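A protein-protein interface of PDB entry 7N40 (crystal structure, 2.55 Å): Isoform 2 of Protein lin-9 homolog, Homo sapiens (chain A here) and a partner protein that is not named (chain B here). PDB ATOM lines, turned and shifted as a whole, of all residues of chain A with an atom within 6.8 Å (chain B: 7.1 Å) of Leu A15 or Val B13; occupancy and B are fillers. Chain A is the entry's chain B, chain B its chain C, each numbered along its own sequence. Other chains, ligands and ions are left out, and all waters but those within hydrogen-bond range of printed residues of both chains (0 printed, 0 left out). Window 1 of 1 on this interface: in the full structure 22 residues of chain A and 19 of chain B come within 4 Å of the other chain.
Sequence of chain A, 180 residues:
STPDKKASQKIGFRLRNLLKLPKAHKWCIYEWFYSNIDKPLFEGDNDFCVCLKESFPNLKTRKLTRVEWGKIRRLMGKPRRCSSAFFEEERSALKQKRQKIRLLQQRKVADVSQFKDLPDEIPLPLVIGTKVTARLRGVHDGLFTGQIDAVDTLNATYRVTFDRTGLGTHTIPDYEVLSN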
ATOM      1  N   LYS A  10      18.800   7.926 -26.482  1.00  0.00           N
ATOM      2  CA  LYS A  10      19.838   8.110 -27.493  1.00  0.00           C
ATOM      3  C   LYS A  10      21.230   8.150 -26.876  1.00  0.00           C
ATOM      4  O   LYS A  10      22.194   7.680 -27.494  1.00  0.00           O
ATOM      5  CB  LYS A  10      19.577   9.384 -28.296  1.00  0.00           C
ATOM      6  CG  LYS A  10      18.538   9.227 -29.420  1.00  0.00           C
ATOM      7  CD  LYS A  10      17.397  10.223 -29.298  1.00  0.00           C
ATOM      8  CE  LYS A  10      17.652  11.467 -30.143  1.00  0.00           C
ATOM      9  NZ  LYS A  10      16.452  12.358 -30.294  1.00  0.00           N
ATOM     10  N   ILE A  11      21.361   8.711 -25.669  1.00  0.00           N
ATOM     11  CA  ILE A  11      22.648   8.683 -24.975  1.00  0.00           C
ATOM     12  C   ILE A  11      23.054   7.243 -24.687  1.00  0.00           C
ATOM     13  O   ILE A  11      24.232   6.879 -24.793  1.00  0.00           O
ATOM     14  CB  ILE A  11      22.586   9.514 -23.680  1.00  0.00           C
ATOM     15  CG1 ILE A  11      22.370  10.997 -23.967  1.00  0.00           C
ATOM     16  CG2 ILE A  11      23.850   9.310 -22.858  1.00  0.00           C
ATOM     17  CD1 ILE A  11      21.737  11.723 -22.817  1.00  0.00           C
ATOM     18  N   GLY A  12      22.081   6.404 -24.320  1.00  0.00           N
ATOM     19  CA  GLY A  12      22.376   5.008 -24.046  1.00  0.00           C
ATOM     20  C   GLY A  12      22.786   4.245 -25.289  1.00  0.00           C
ATOM     21  O   GLY A  12      23.689   3.401 -25.240  1.00  0.00           O
ATOM     22  N   PHE A  13      22.136   4.531 -26.421  1.00  0.00           N
ATOM     23  CA  PHE A  13      22.547   3.908 -27.676  1.00  0.00           C
ATOM     24  C   PHE A  13      24.013   4.215 -27.984  1.00  0.00           C
ATOM     25  O   PHE A  13      24.777   3.317 -28.360  1.00  0.00           O
ATOM     26  CB  PHE A  13      21.621   4.367 -28.811  1.00  0.00           C
ATOM     27  CG  PHE A  13      22.116   4.024 -30.208  1.00  0.00           C
ATOM     28  CD1 PHE A  13      21.861   2.777 -30.772  1.00  0.00           C
ATOM     29  CD2 PHE A  13      22.798   4.970 -30.976  1.00  0.00           C
ATOM     30  CE1 PHE A  13      22.300   2.469 -32.060  1.00  0.00           C
ATOM     31  CE2 PHE A  13      23.234   4.669 -32.263  1.00  0.00           C
ATOM     32  CZ  PHE A  13      22.986   3.417 -32.802  1.00  0.00           C
ATOM     33  N   ARG A  14      24.430   5.473 -27.794  1.00  0.00           N
ATOM     34  CA  ARG A  14      25.828   5.842 -27.983  1.00  0.00           C
ATOM     35  C   ARG A  14      26.732   5.101 -27.003  1.00  0.00           C
ATOM     36  O   ARG A  14      27.801   4.604 -27.380  1.00  0.00           O
ATOM     37  CB  ARG A  14      25.995   7.357 -27.827  1.00  0.00           C
ATOM     38  CG  ARG A  14      26.145   8.147 -29.133  1.00  0.00           C
ATOM     39  CD  ARG A  14      26.907   9.464 -28.908  1.00  0.00           C
ATOM     40  NE  ARG A  14      26.250  10.258 -27.877  1.00  0.00           N
ATOM     41  CZ  ARG A  14      26.879  10.996 -26.974  1.00  0.00           C
ATOM     42  NH1 ARG A  14      28.200  11.072 -26.972  1.00  0.00           N
ATOM     43  NH2 ARG A  14      26.178  11.672 -26.075  1.00  0.00           N
ATOM     44  N   LEU A  15      26.321   5.012 -25.738  1.00  0.00           N
ATOM     45  CA  LEU A  15      27.169   4.347 -24.757  1.00  0.00           C
ATOM     46  C   LEU A  15      27.316   2.872 -25.081  1.00  0.00           C
ATOM     47  O   LEU A  15      28.424   2.326 -25.036  1.00  0.00           O
ATOM     48  CB  LEU A  15      26.602   4.516 -23.354  1.00  0.00           C
ATOM     49  CG  LEU A  15      27.429   3.780 -22.300  1.00  0.00           C
ATOM     50  CD1 LEU A  15      28.859   4.352 -22.223  1.00  0.00           C
ATOM     51  CD2 LEU A  15      26.735   3.799 -20.947  1.00  0.00           C
ATOM     52  N   ARG A  16      26.203   2.217 -25.426  1.00  0.00           N
ATOM     53  CA  ARG A  16      26.223   0.784 -25.716  1.00  0.00           C
ATOM     54  C   ARG A  16      27.120   0.453 -26.906  1.00  0.00           C
ATOM     55  O   ARG A  16      27.709  -0.634 -26.950  1.00  0.00           O
ATOM     56  CB  ARG A  16      24.795   0.282 -25.962  1.00  0.00           C
ATOM     57  CG  ARG A  16      24.657  -1.208 -26.177  1.00  0.00           C
ATOM     58  CD  ARG A  16      23.194  -1.643 -26.094  1.00  0.00           C
ATOM     59  NE  ARG A  16      22.944  -2.925 -26.756  1.00  0.00           N
ATOM     60  CZ  ARG A  16      22.914  -4.102 -26.135  1.00  0.00           C
ATOM     61  NH1 ARG A  16      23.116  -4.178 -24.825  1.00  0.00           N
ATOM     62  NH2 ARG A  16      22.685  -5.210 -26.825  1.00  0.00           N
ATOM     63  N   ASN A  17      27.267   1.383 -27.858  1.00  0.00           N
ATOM     64  CA  ASN A  17      28.084   1.108 -29.037  1.00  0.00           C
ATOM     65  C   ASN A  17      29.570   1.101 -28.718  1.00  0.00           C
ATOM     66  O   ASN A  17      30.330   0.312 -29.293  1.00  0.00           O
ATOM     67  CB  ASN A  17      27.786   2.126 -30.120  1.00  0.00           C
ATOM     68  CG  ASN A  17      26.453   1.899 -30.737  1.00  0.00           C
ATOM     69  OD1 ASN A  17      25.958   0.765 -30.742  1.00  0.00           O
ATOM     70  ND2 ASN A  17      25.847   2.963 -31.270  1.00  0.00           N
ATOM     71  N   LEU A  18      30.007   1.987 -27.824  1.00  0.00           N
ATOM     72  CA  LEU A  18      31.377   1.924 -27.335  1.00  0.00           C
ATOM     73  C   LEU A  18      31.598   0.652 -26.525  1.00  0.00           C
ATOM     74  O   LEU A  18      32.559  -0.089 -26.764  1.00  0.00           O
ATOM     75  CB  LEU A  18      31.691   3.163 -26.496  1.00  0.00           C
ATOM     76  CG  LEU A  18      33.128   3.335 -26.028  1.00  0.00           C
ATOM     77  CD1 LEU A  18      33.473   4.825 -25.855  1.00  0.00           C
ATOM     78  CD2 LEU A  18      33.357   2.567 -24.738  1.00  0.00           C
ATOM     79  N   LEU A  19      30.720   0.395 -25.546  1.00  0.00           N
ATOM     80  CA  LEU A  19      30.964  -0.674 -24.589  1.00  0.00           C
ATOM     81  C   LEU A  19      30.882  -2.051 -25.237  1.00  0.00           C
ATOM     82  O   LEU A  19      31.541  -2.986 -24.775  1.00  0.00           O
ATOM     83  CB  LEU A  19      29.976  -0.565 -23.433  1.00  0.00           C
ATOM     84  CG  LEU A  19      30.168   0.611 -22.483  1.00  0.00           C
ATOM     85  CD1 LEU A  19      29.020   0.640 -21.497  1.00  0.00           C
ATOM     86  CD2 LEU A  19      31.507   0.502 -21.756  1.00  0.00           C
ATOM     87  N   LYS A  20      30.086  -2.200 -26.301  1.00  0.00           N
ATOM     88  CA  LYS A  20      30.021  -3.478 -27.000  1.00  0.00           C
ATOM     89  C   LYS A  20      31.336  -3.812 -27.695  1.00  0.00           C
ATOM     90  O   LYS A  20      31.581  -4.988 -27.994  1.00  0.00           O
ATOM     91  CB  LYS A  20      28.877  -3.475 -28.021  1.00  0.00           C
ATOM     92  CG  LYS A  20      29.267  -2.873 -29.378  1.00  0.00           C
ATOM     93  CD  LYS A  20      28.080  -2.267 -30.069  1.00  0.00           C
ATOM     94  CE  LYS A  20      28.209  -2.308 -31.562  1.00  0.00           C
ATOM     95  NZ  LYS A  20      26.835  -2.161 -32.150  1.00  0.00           N
ATOM     96  N   CYS A  28      38.071   1.025 -20.620  1.00  0.00           N
ATOM     97  CA  CYS A  28      37.316   1.528 -19.474  1.00  0.00           C
ATOM     98  C   CYS A  28      37.843   0.962 -18.169  1.00  0.00           C
ATOM     99  O   CYS A  28      37.865   1.666 -17.148  1.00  0.00           O
ATOM    100  CB  CYS A  28      35.837   1.180 -19.625  1.00  0.00           C
ATOM    101  SG  CYS A  28      34.973   2.151 -20.871  1.00  0.00           S
ATOM    102  N   TYR B   4      16.614   8.483 -14.966  1.00  0.00           N
ATOM    103  CA  TYR B   4      16.697   7.514 -16.063  1.00  0.00           C
ATOM    104  C   TYR B   4      17.878   6.555 -15.962  1.00  0.00           C
ATOM    105  O   TYR B   4      18.948   6.847 -16.489  1.00  0.00           O
ATOM    106  CB  TYR B   4      16.793   8.233 -17.401  1.00  0.00           C
ATOM    107  CG  TYR B   4      16.457   7.340 -18.567  1.00  0.00           C
ATOM    108  CD1 TYR B   4      15.139   7.044 -18.874  1.00  0.00           C
ATOM    109  CD2 TYR B   4      17.455   6.771 -19.347  1.00  0.00           C
ATOM    110  CE1 TYR B   4      14.815   6.218 -19.936  1.00  0.00           C
ATOM    111  CE2 TYR B   4      17.143   5.951 -20.423  1.00  0.00           C
ATOM    112  CZ  TYR B   4      15.816   5.676 -20.710  1.00  0.00           C
ATOM    113  OH  TYR B   4      15.472   4.864 -21.767  1.00  0.00           O
ATOM    114  N   VAL B   5      17.705   5.400 -15.321  1.00  0.00           N
ATOM    115  CA  VAL B   5      18.816   4.485 -15.079  1.00  0.00           C
ATOM    116  C   VAL B   5      18.685   3.274 -15.993  1.00  0.00           C
ATOM    117  O   VAL B   5      17.604   2.690 -16.117  1.00  0.00           O
ATOM    118  CB  VAL B   5      18.900   4.059 -13.605  1.00  0.00           C
ATOM    119  CG1 VAL B   5      17.597   3.436 -13.135  1.00  0.00           C
ATOM    120  CG2 VAL B   5      20.054   3.098 -13.426  1.00  0.00           C
ATOM    121  N   ILE B   6      19.793   2.899 -16.629  1.00  0.00           N
ATOM    122  CA  ILE B   6      19.830   1.751 -17.519  1.00  0.00           C
ATOM    123  C   ILE B   6      20.857   0.751 -17.001  1.00  0.00           C
ATOM    124  O   ILE B   6      21.798   1.091 -16.281  1.00  0.00           O
ATOM    125  CB  ILE B   6      20.144   2.147 -18.976  1.00  0.00           C
ATOM    126  CG1 ILE B   6      21.649   2.313 -19.182  1.00  0.00           C
ATOM    127  CG2 ILE B   6      19.415   3.425 -19.360  1.00  0.00           C
ATOM    128  CD1 ILE B   6      22.044   2.345 -20.656  1.00  0.00           C
ATOM    129  N   LYS B   7      20.646  -0.509 -17.362  1.00  0.00           N
ATOM    130  CA  LYS B   7      21.593  -1.578 -17.100  1.00  0.00           C
ATOM    131  C   LYS B   7      22.290  -1.917 -18.407  1.00  0.00           C
ATOM    132  O   LYS B   7      21.634  -2.111 -19.434  1.00  0.00           O
ATOM    133  CB  LYS B   7      20.892  -2.810 -16.525  1.00  0.00           C
ATOM    134  CG  LYS B   7      19.807  -2.485 -15.503  1.00  0.00           C
ATOM    135  CD  LYS B   7      18.508  -3.239 -15.792  1.00  0.00           C
ATOM    136  CE  LYS B   7      17.345  -2.655 -15.007  1.00  0.00           C
ATOM    137  NZ  LYS B   7      16.035  -3.044 -15.588  1.00  0.00           N
ATOM    138  N   LEU B   8      23.617  -1.966 -18.371  1.00  0.00           N
ATOM    139  CA  LEU B   8      24.421  -2.225 -19.564  1.00  0.00           C
ATOM    140  C   LEU B   8      25.626  -3.045 -19.129  1.00  0.00           C
ATOM    141  O   LEU B   8      26.557  -2.501 -18.530  1.00  0.00           O
ATOM    142  CB  LEU B   8      24.852  -0.925 -20.240  1.00  0.00           C
ATOM    143  CG  LEU B   8      24.246  -0.598 -21.607  1.00  0.00           C
ATOM    144  CD1 LEU B   8      25.047   0.493 -22.282  1.00  0.00           C
ATOM    145  CD2 LEU B   8      24.172  -1.838 -22.492  1.00  0.00           C
ATOM    146  N   PHE B   9      25.592  -4.347 -19.420  1.00  0.00           N
ATOM    147  CA  PHE B   9      26.709  -5.262 -19.170  1.00  0.00           C
ATOM    148  C   PHE B   9      27.145  -5.242 -17.698  1.00  0.00           C
ATOM    149  O   PHE B   9      28.285  -4.909 -17.357  1.00  0.00           O
ATOM    150  CB  PHE B   9      27.881  -4.948 -20.109  1.00  0.00           C
ATOM    151  CG  PHE B   9      27.477  -4.760 -21.553  1.00  0.00           C
ATOM    152  CD1 PHE B   9      26.731  -5.718 -22.214  1.00  0.00           C
ATOM    153  CD2 PHE B   9      27.847  -3.627 -22.249  1.00  0.00           C
ATOM    154  CE1 PHE B   9      26.363  -5.541 -23.540  1.00  0.00           C
ATOM    155  CE2 PHE B   9      27.480  -3.450 -23.570  1.00  0.00           C
ATOM    156  CZ  PHE B   9      26.736  -4.411 -24.213  1.00  0.00           C
ATOM    157  N   ARG B  11      26.774  -3.382 -15.279  1.00  0.00           N
ATOM    158  CA  ARG B  11      26.890  -2.104 -14.590  1.00  0.00           C
ATOM    159  C   ARG B  11      25.729  -1.203 -14.983  1.00  0.00           C
ATOM    160  O   ARG B  11      25.157  -1.341 -16.068  1.00  0.00           O
ATOM    161  CB  ARG B  11      28.209  -1.400 -14.909  1.00  0.00           C
ATOM    162  CG  ARG B  11      29.435  -2.250 -14.684  1.00  0.00           C
ATOM    163  CD  ARG B  11      30.678  -1.382 -14.625  1.00  0.00           C
ATOM    164  NE  ARG B  11      30.775  -0.686 -13.349  1.00  0.00           N
ATOM    165  CZ  ARG B  11      31.348  -1.205 -12.271  1.00  0.00           C
ATOM    166  NH1 ARG B  11      31.873  -2.426 -12.318  1.00  0.00           N
ATOM    167  NH2 ARG B  11      31.391  -0.502 -11.148  1.00  0.00           N
ATOM    168  N   SER B  12      25.389  -0.272 -14.096  1.00  0.00           N
ATOM    169  CA  SER B  12      24.293   0.653 -14.329  1.00  0.00           C
ATOM    170  C   SER B  12      24.801   2.088 -14.285  1.00  0.00           C
ATOM    171  O   SER B  12      25.864   2.383 -13.731  1.00  0.00           O
ATOM    172  CB  SER B  12      23.162   0.455 -13.307  1.00  0.00           C
ATOM    173  OG  SER B  12      23.621   0.632 -11.980  1.00  0.00           O
ATOM    174  N   VAL B  13      24.017   2.974 -14.890  1.00  0.00           N
ATOM    175  CA  VAL B  13      24.370   4.380 -15.013  1.00  0.00           C
ATOM    176  C   VAL B  13      23.080   5.171 -15.183  1.00  0.00           C
ATOM    177  O   VAL B  13      22.177   4.759 -15.916  1.00  0.00           O
ATOM    178  CB  VAL B  13      25.347   4.604 -16.189  1.00  0.00           C
ATOM    179  CG1 VAL B  13      24.817   3.952 -17.455  1.00  0.00           C
ATOM    180  CG2 VAL B  13      25.598   6.083 -16.415  1.00  0.00           C
ATOM    181  N   ASP B  14      22.983   6.295 -14.482  1.00  0.00           N
ATOM    182  CA  ASP B  14      21.846   7.198 -14.649  1.00  0.00           C
ATOM    183  C   ASP B  14      22.205   8.201 -15.734  1.00  0.00           C
ATOM    184  O   ASP B  14      22.948   9.155 -15.494  1.00  0.00           O
ATOM    185  CB  ASP B  14      21.488   7.904 -13.345  1.00  0.00           C
ATOM    186  CG  ASP B  14      20.395   8.950 -13.539  1.00  0.00           C
ATOM    187  OD1 ASP B  14      19.491   8.713 -14.368  1.00  0.00           O
ATOM    188  OD2 ASP B  14      20.438  10.011 -12.869  1.00  0.00           O
ATOM    189  N   LEU B  15      21.686   7.987 -16.937  1.00  0.00           N
ATOM    190  CA  LEU B  15      21.993   8.920 -18.010  1.00  0.00           C
ATOM    191  C   LEU B  15      21.180  10.201 -17.926  1.00  0.00           C
ATOM    192  O   LEU B  15      21.298  11.048 -18.808  1.00  0.00           O
ATOM    193  CB  LEU B  15      21.777   8.226 -19.353  1.00  0.00           C
ATOM    194  CG  LEU B  15      22.697   7.016 -19.433  1.00  0.00           C
ATOM    195  CD1 LEU B  15      22.152   6.008 -20.418  1.00  0.00           C
ATOM    196  CD2 LEU B  15      24.109   7.456 -19.785  1.00  0.00           C
ATOM    197  N   ALA B  16      20.343  10.370 -16.903  1.00  0.00           N
ATOM    198  CA  ALA B  16      19.520  11.575 -16.824  1.00  0.00           C
ATOM    199  C   ALA B  16      20.359  12.822 -16.545  1.00  0.00           C
ATOM    200  O   ALA B  16      19.977  13.931 -16.939  1.00  0.00           O
ATOM    201  CB  ALA B  16      18.429  11.408 -15.759  1.00  0.00           C
ATOM    202  N   GLN B  17      21.504  12.669 -15.877  1.00  0.00           N
ATOM    203  CA  GLN B  17      22.377  13.814 -15.630  1.00  0.00           C
ATOM    204  C   GLN B  17      23.121  14.277 -16.877  1.00  0.00           C
ATOM    205  O   GLN B  17      23.807  15.304 -16.826  1.00  0.00           O
ATOM    206  CB  GLN B  17      23.390  13.471 -14.540  1.00  0.00           C
ATOM    207  CG  GLN B  17      24.228  12.229 -14.851  1.00  0.00           C
ATOM    208  CD  GLN B  17      25.552  12.206 -14.101  1.00  0.00           C
ATOM    209  OE1 GLN B  17      26.185  13.247 -13.905  1.00  0.00           O
ATOM    210  NE2 GLN B  17      25.972  11.017 -13.672  1.00  0.00           N
ATOM    211  N   PHE B  18      23.029  13.548 -17.982  1.00  0.00           N
ATOM    212  CA  PHE B  18      23.760  13.896 -19.190  1.00  0.00           C
ATOM    213  C   PHE B  18      22.800  14.395 -20.256  1.00  0.00           C
ATOM    214  O   PHE B  18      21.580  14.333 -20.114  1.00  0.00           O
ATOM    215  CB  PHE B  18      24.567  12.704 -19.728  1.00  0.00           C
ATOM    216  CG  PHE B  18      25.521  12.112 -18.727  1.00  0.00           C
ATOM    217  CD1 PHE B  18      26.688  12.762 -18.396  1.00  0.00           C
ATOM    218  CD2 PHE B  18      25.241  10.901 -18.115  1.00  0.00           C
ATOM    219  CE1 PHE B  18      27.573  12.210 -17.476  1.00  0.00           C
ATOM    220  CE2 PHE B  18      26.113  10.350 -17.185  1.00  0.00           C
ATOM    221  CZ  PHE B  18      27.278  11.004 -16.867  1.00  0.00           C
ATOM    222  N   LEU B  24      31.513  10.965 -24.599  1.00  0.00           N
ATOM    223  CA  LEU B  24      31.407   9.665 -23.948  1.00  0.00           C
ATOM    224  C   LEU B  24      32.351   9.501 -22.764  1.00  0.00           C
ATOM    225  O   LEU B  24      32.064   8.681 -21.894  1.00  0.00           O
ATOM    226  CB  LEU B  24      31.657   8.548 -24.947  1.00  0.00           C
ATOM    227  CG  LEU B  24      30.402   8.129 -25.708  1.00  0.00           C
ATOM    228  CD1 LEU B  24      30.778   7.273 -26.895  1.00  0.00           C
ATOM    229  CD2 LEU B  24      29.455   7.370 -24.803  1.00  0.00           C
ATOM    230  N   PRO B  26      32.976  11.284 -19.900  1.00  0.00           N
ATOM    231  CA  PRO B  26      32.360  11.356 -18.562  1.00  0.00           C
ATOM    232  C   PRO B  26      31.227  10.358 -18.358  1.00  0.00           C
ATOM    233  O   PRO B  26      30.923  10.014 -17.204  1.00  0.00           O
ATOM    234  CB  PRO B  26      31.859  12.802 -18.481  1.00  0.00           C
ATOM    235  CG  PRO B  26      31.715  13.241 -19.932  1.00  0.00           C
ATOM    236  CD  PRO B  26      32.822  12.551 -20.646  1.00  0.00           C
ATOM    237  N   ILE B  27      30.603   9.872 -19.437  1.00  0.00           N
ATOM    238  CA  ILE B  27      29.516   8.910 -19.293  1.00  0.00           C
ATOM    239  C   ILE B  27      30.068   7.521 -18.994  1.00  0.00           C
ATOM    240  O   ILE B  27      29.506   6.774 -18.183  1.00  0.00           O
ATOM    241  CB  ILE B  27      28.641   8.938 -20.556  1.00  0.00           C
ATOM    242  CG1 ILE B  27      27.988  10.318 -20.705  1.00  0.00           C
ATOM    243  CG2 ILE B  27      27.591   7.846 -20.528  1.00  0.00           C
ATOM    244  CD1 ILE B  27      27.280  10.512 -22.035  1.00  0.00           C
ATOM    245  N   CYS B  28      31.188   7.167 -19.629  1.00  0.00           N
ATOM    246  CA  CYS B  28      31.905   5.938 -19.290  1.00  0.00           C
ATOM    247  C   CYS B  28      32.281   5.902 -17.819  1.00  0.00           C
ATOM    248  O   CYS B  28      32.141   4.861 -17.157  1.00  0.00           O
ATOM    249  CB  CYS B  28      33.164   5.816 -20.141  1.00  0.00           C
ATOM    250  SG  CYS B  28      32.846   5.466 -21.898  1.00  0.00           S
ATOM    251  N   ARG B  29      32.776   7.030 -17.299  1.00  0.00           N
ATOM    252  CA  ARG B  29      33.168   7.099 -15.900  1.00  0.00           C
ATOM    253  C   ARG B  29      32.007   6.742 -14.987  1.00  0.00           C
ATOM    254  O   ARG B  29      32.158   5.931 -14.060  1.00  0.00           O
ATOM    255  CB  ARG B  29      33.683   8.494 -15.575  1.00  0.00           C
ATOM    256  CG  ARG B  29      33.989   8.705 -14.099  1.00  0.00           C
ATOM    257  CD  ARG B  29      34.794   9.964 -13.915  1.00  0.00           C
ATOM    258  NE  ARG B  29      34.043  11.112 -14.401  1.00  0.00           N
ATOM    259  CZ  ARG B  29      34.568  12.163 -15.010  1.00  0.00           C
ATOM    260  NH1 ARG B  29      35.864  12.247 -15.248  1.00  0.00           N
ATOM    261  NH2 ARG B  29      33.776  13.136 -15.389  1.00  0.00           N
ATOM    262  N   ALA B  30      30.837   7.346 -15.233  1.00  0.00           N
ATOM    263  CA  ALA B  30      29.663   7.075 -14.405  1.00  0.00           C
ATOM    264  C   ALA B  30      29.236   5.621 -14.536  1.00  0.00           C
ATOM    265  O   ALA B  30      28.771   4.998 -13.567  1.00  0.00           O
ATOM    266  CB  ALA B  30      28.514   8.005 -14.793  1.00  0.00           C
ATOM    267  N   TRP B  31      29.393   5.064 -15.736  1.00  0.00           N
ATOM    268  CA  TRP B  31      29.136   3.646 -15.912  1.00  0.00           C
ATOM    269  C   TRP B  31      30.099   2.808 -15.075  1.00  0.00           C
ATOM    270  O   TRP B  31      29.705   1.782 -14.515  1.00  0.00           O
ATOM    271  CB  TRP B  31      29.232   3.291 -17.393  1.00  0.00           C
ATOM    272  CG  TRP B  31      28.932   1.859 -17.647  1.00  0.00           C
ATOM    273  CD1 TRP B  31      27.697   1.277 -17.724  1.00  0.00           C
ATOM    274  CD2 TRP B  31      29.879   0.819 -17.853  1.00  0.00           C
ATOM    275  NE1 TRP B  31      27.822  -0.064 -17.977  1.00  0.00           N
ATOM    276  CE2 TRP B  31      29.154  -0.372 -18.055  1.00  0.00           C
ATOM    277  CE3 TRP B  31      31.272   0.777 -17.898  1.00  0.00           C
ATOM    278  CZ2 TRP B  31      29.776  -1.595 -18.281  1.00  0.00           C
ATOM    279  CZ3 TRP B  31      31.889  -0.439 -18.123  1.00  0.00           C
ATOM    280  CH2 TRP B  31      31.141  -1.607 -18.313  1.00  0.00           C
ATOM    281  N   MET B  32      31.360   3.248 -14.938  1.00  0.00           N
ATOM    282  CA  MET B  32      32.339   2.445 -14.205  1.00  0.00           C
ATOM    283  C   MET B  32      32.250   2.639 -12.691  1.00  0.00           C
ATOM    284  O   MET B  32      32.568   1.710 -11.943  1.00  0.00           O
ATOM    285  CB  MET B  32      33.766   2.754 -14.685  1.00  0.00           C
ATOM    286  CG  MET B  32      34.188   2.085 -16.009  1.00  0.00           C
ATOM    287  SD  MET B  32      34.514   0.297 -15.931  1.00  0.00           S
ATOM    288  CE  MET B  32      35.674   0.197 -14.568  1.00  0.00           C
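The side-chain amino group (NZ) of Lys A20 sits at hydrogen-bond distance from the side-chain amide oxygen (OD1) of Asn A17, at 3.4 Å. The backbone carbonyl oxygen of Tyr B4 is in hydrogen-bond range of the backbone NH of Leu B15. N of Ile B6 lies within hydrogen-bond range of O of Val B13 (3.1 Å). The backbone carbonyl oxygen (O) of Leu B8 sits at hydrogen-bond distance from the indole nitrogen (NE1) of Trp B31, at 2.8 Å. The guanidinium group (NE) of Arg B11 is in hydrogen-bond range of the backbone carbonyl oxygen (O) of Trp B31 (2.9 Å). The backbone carbonyl oxygen of Leu B24 is in hydrogen-bond range of the side-chain sulfur of Cys B28.
Among the printed residues, pairs that only touch across the chains: Arg A16 with Leu B8 (3.5 Å), Leu A19 with Trp B31 (3.6 Å), Ile A11 with Leu B15 (3.6 Å), Arg A16 with Phe B9 (3.7 Å), Cys A28 with Met B32 (3.7 Å), Ile A11 with Ile B27 (3.7 Å), Ile A11 with Phe B18 (3.8 Å), Gly A12 with Leu B15 (3.8 Å), Leu A18 with Leu B24 (3.8 Å), Leu A15 with Leu B24 (3.8 Å), Leu A19 with Phe B9 (3.8 Å), Arg A14 with Leu B24 (3.9 Å), Leu A15 with Leu B8 (3.9 Å), Lys A20 with Phe B9 (3.98 Å) and Leu A15 with Val B13 (3.99 Å).
Of the printed residues of chain B, Ile A11 touches Leu B15 (3.6 Å), Phe B18 (3.8 Å) and Ile B27 (3.7 Å). Printed residues of chain B within 4 Å of Leu A15: Leu B8 (3.9 Å), Val B13 (3.99 Å) and Leu B24 (3.8 Å). Of the printed residues of chain B, Arg A16 touches Leu B8 and Phe B9. Printed residues of chain B within 4 Å of Leu A18: Leu B24. Printed residues of chain A within 4 Å of Leu B8: Leu A15 and Arg A16. Of the printed residues of chain A, Val B13 touches Leu A15 (3.99 Å). Of the printed residues of chain A, Ile B27 touches Ile A11. The nearest printed residue of chain A that does not touch Phe B18 is Arg A14 (6.6 Å).
Of the 12 printed residues of chain A, 9 touch a printed residue of chain B. Printed residues of chain A that touch a printed residue of chain B: Ile A11, Gly A12, Arg A14, Leu A15, Arg A16, Leu A18, Leu A19, Lys A20 and Cys A28. Hydrophobic or aromatic side chains of chain A that line the printed part of chain B: Ile A11, Leu A15, Leu A18 and Leu A19. Hydrophobic or aromatic side chains of chain B within 4 Å of the printed part of chain A: Leu B8, Phe B9, Val B13, Leu B15, Leu B24, Ile B27, Trp B31 and Met B32. Among the printed residues, 15 pairs touch across the chains. Among the printed residues, no Asp or Glu carboxylate lies within 4 Å of a Lys or Arg side-chain nitrogen of the other chain.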
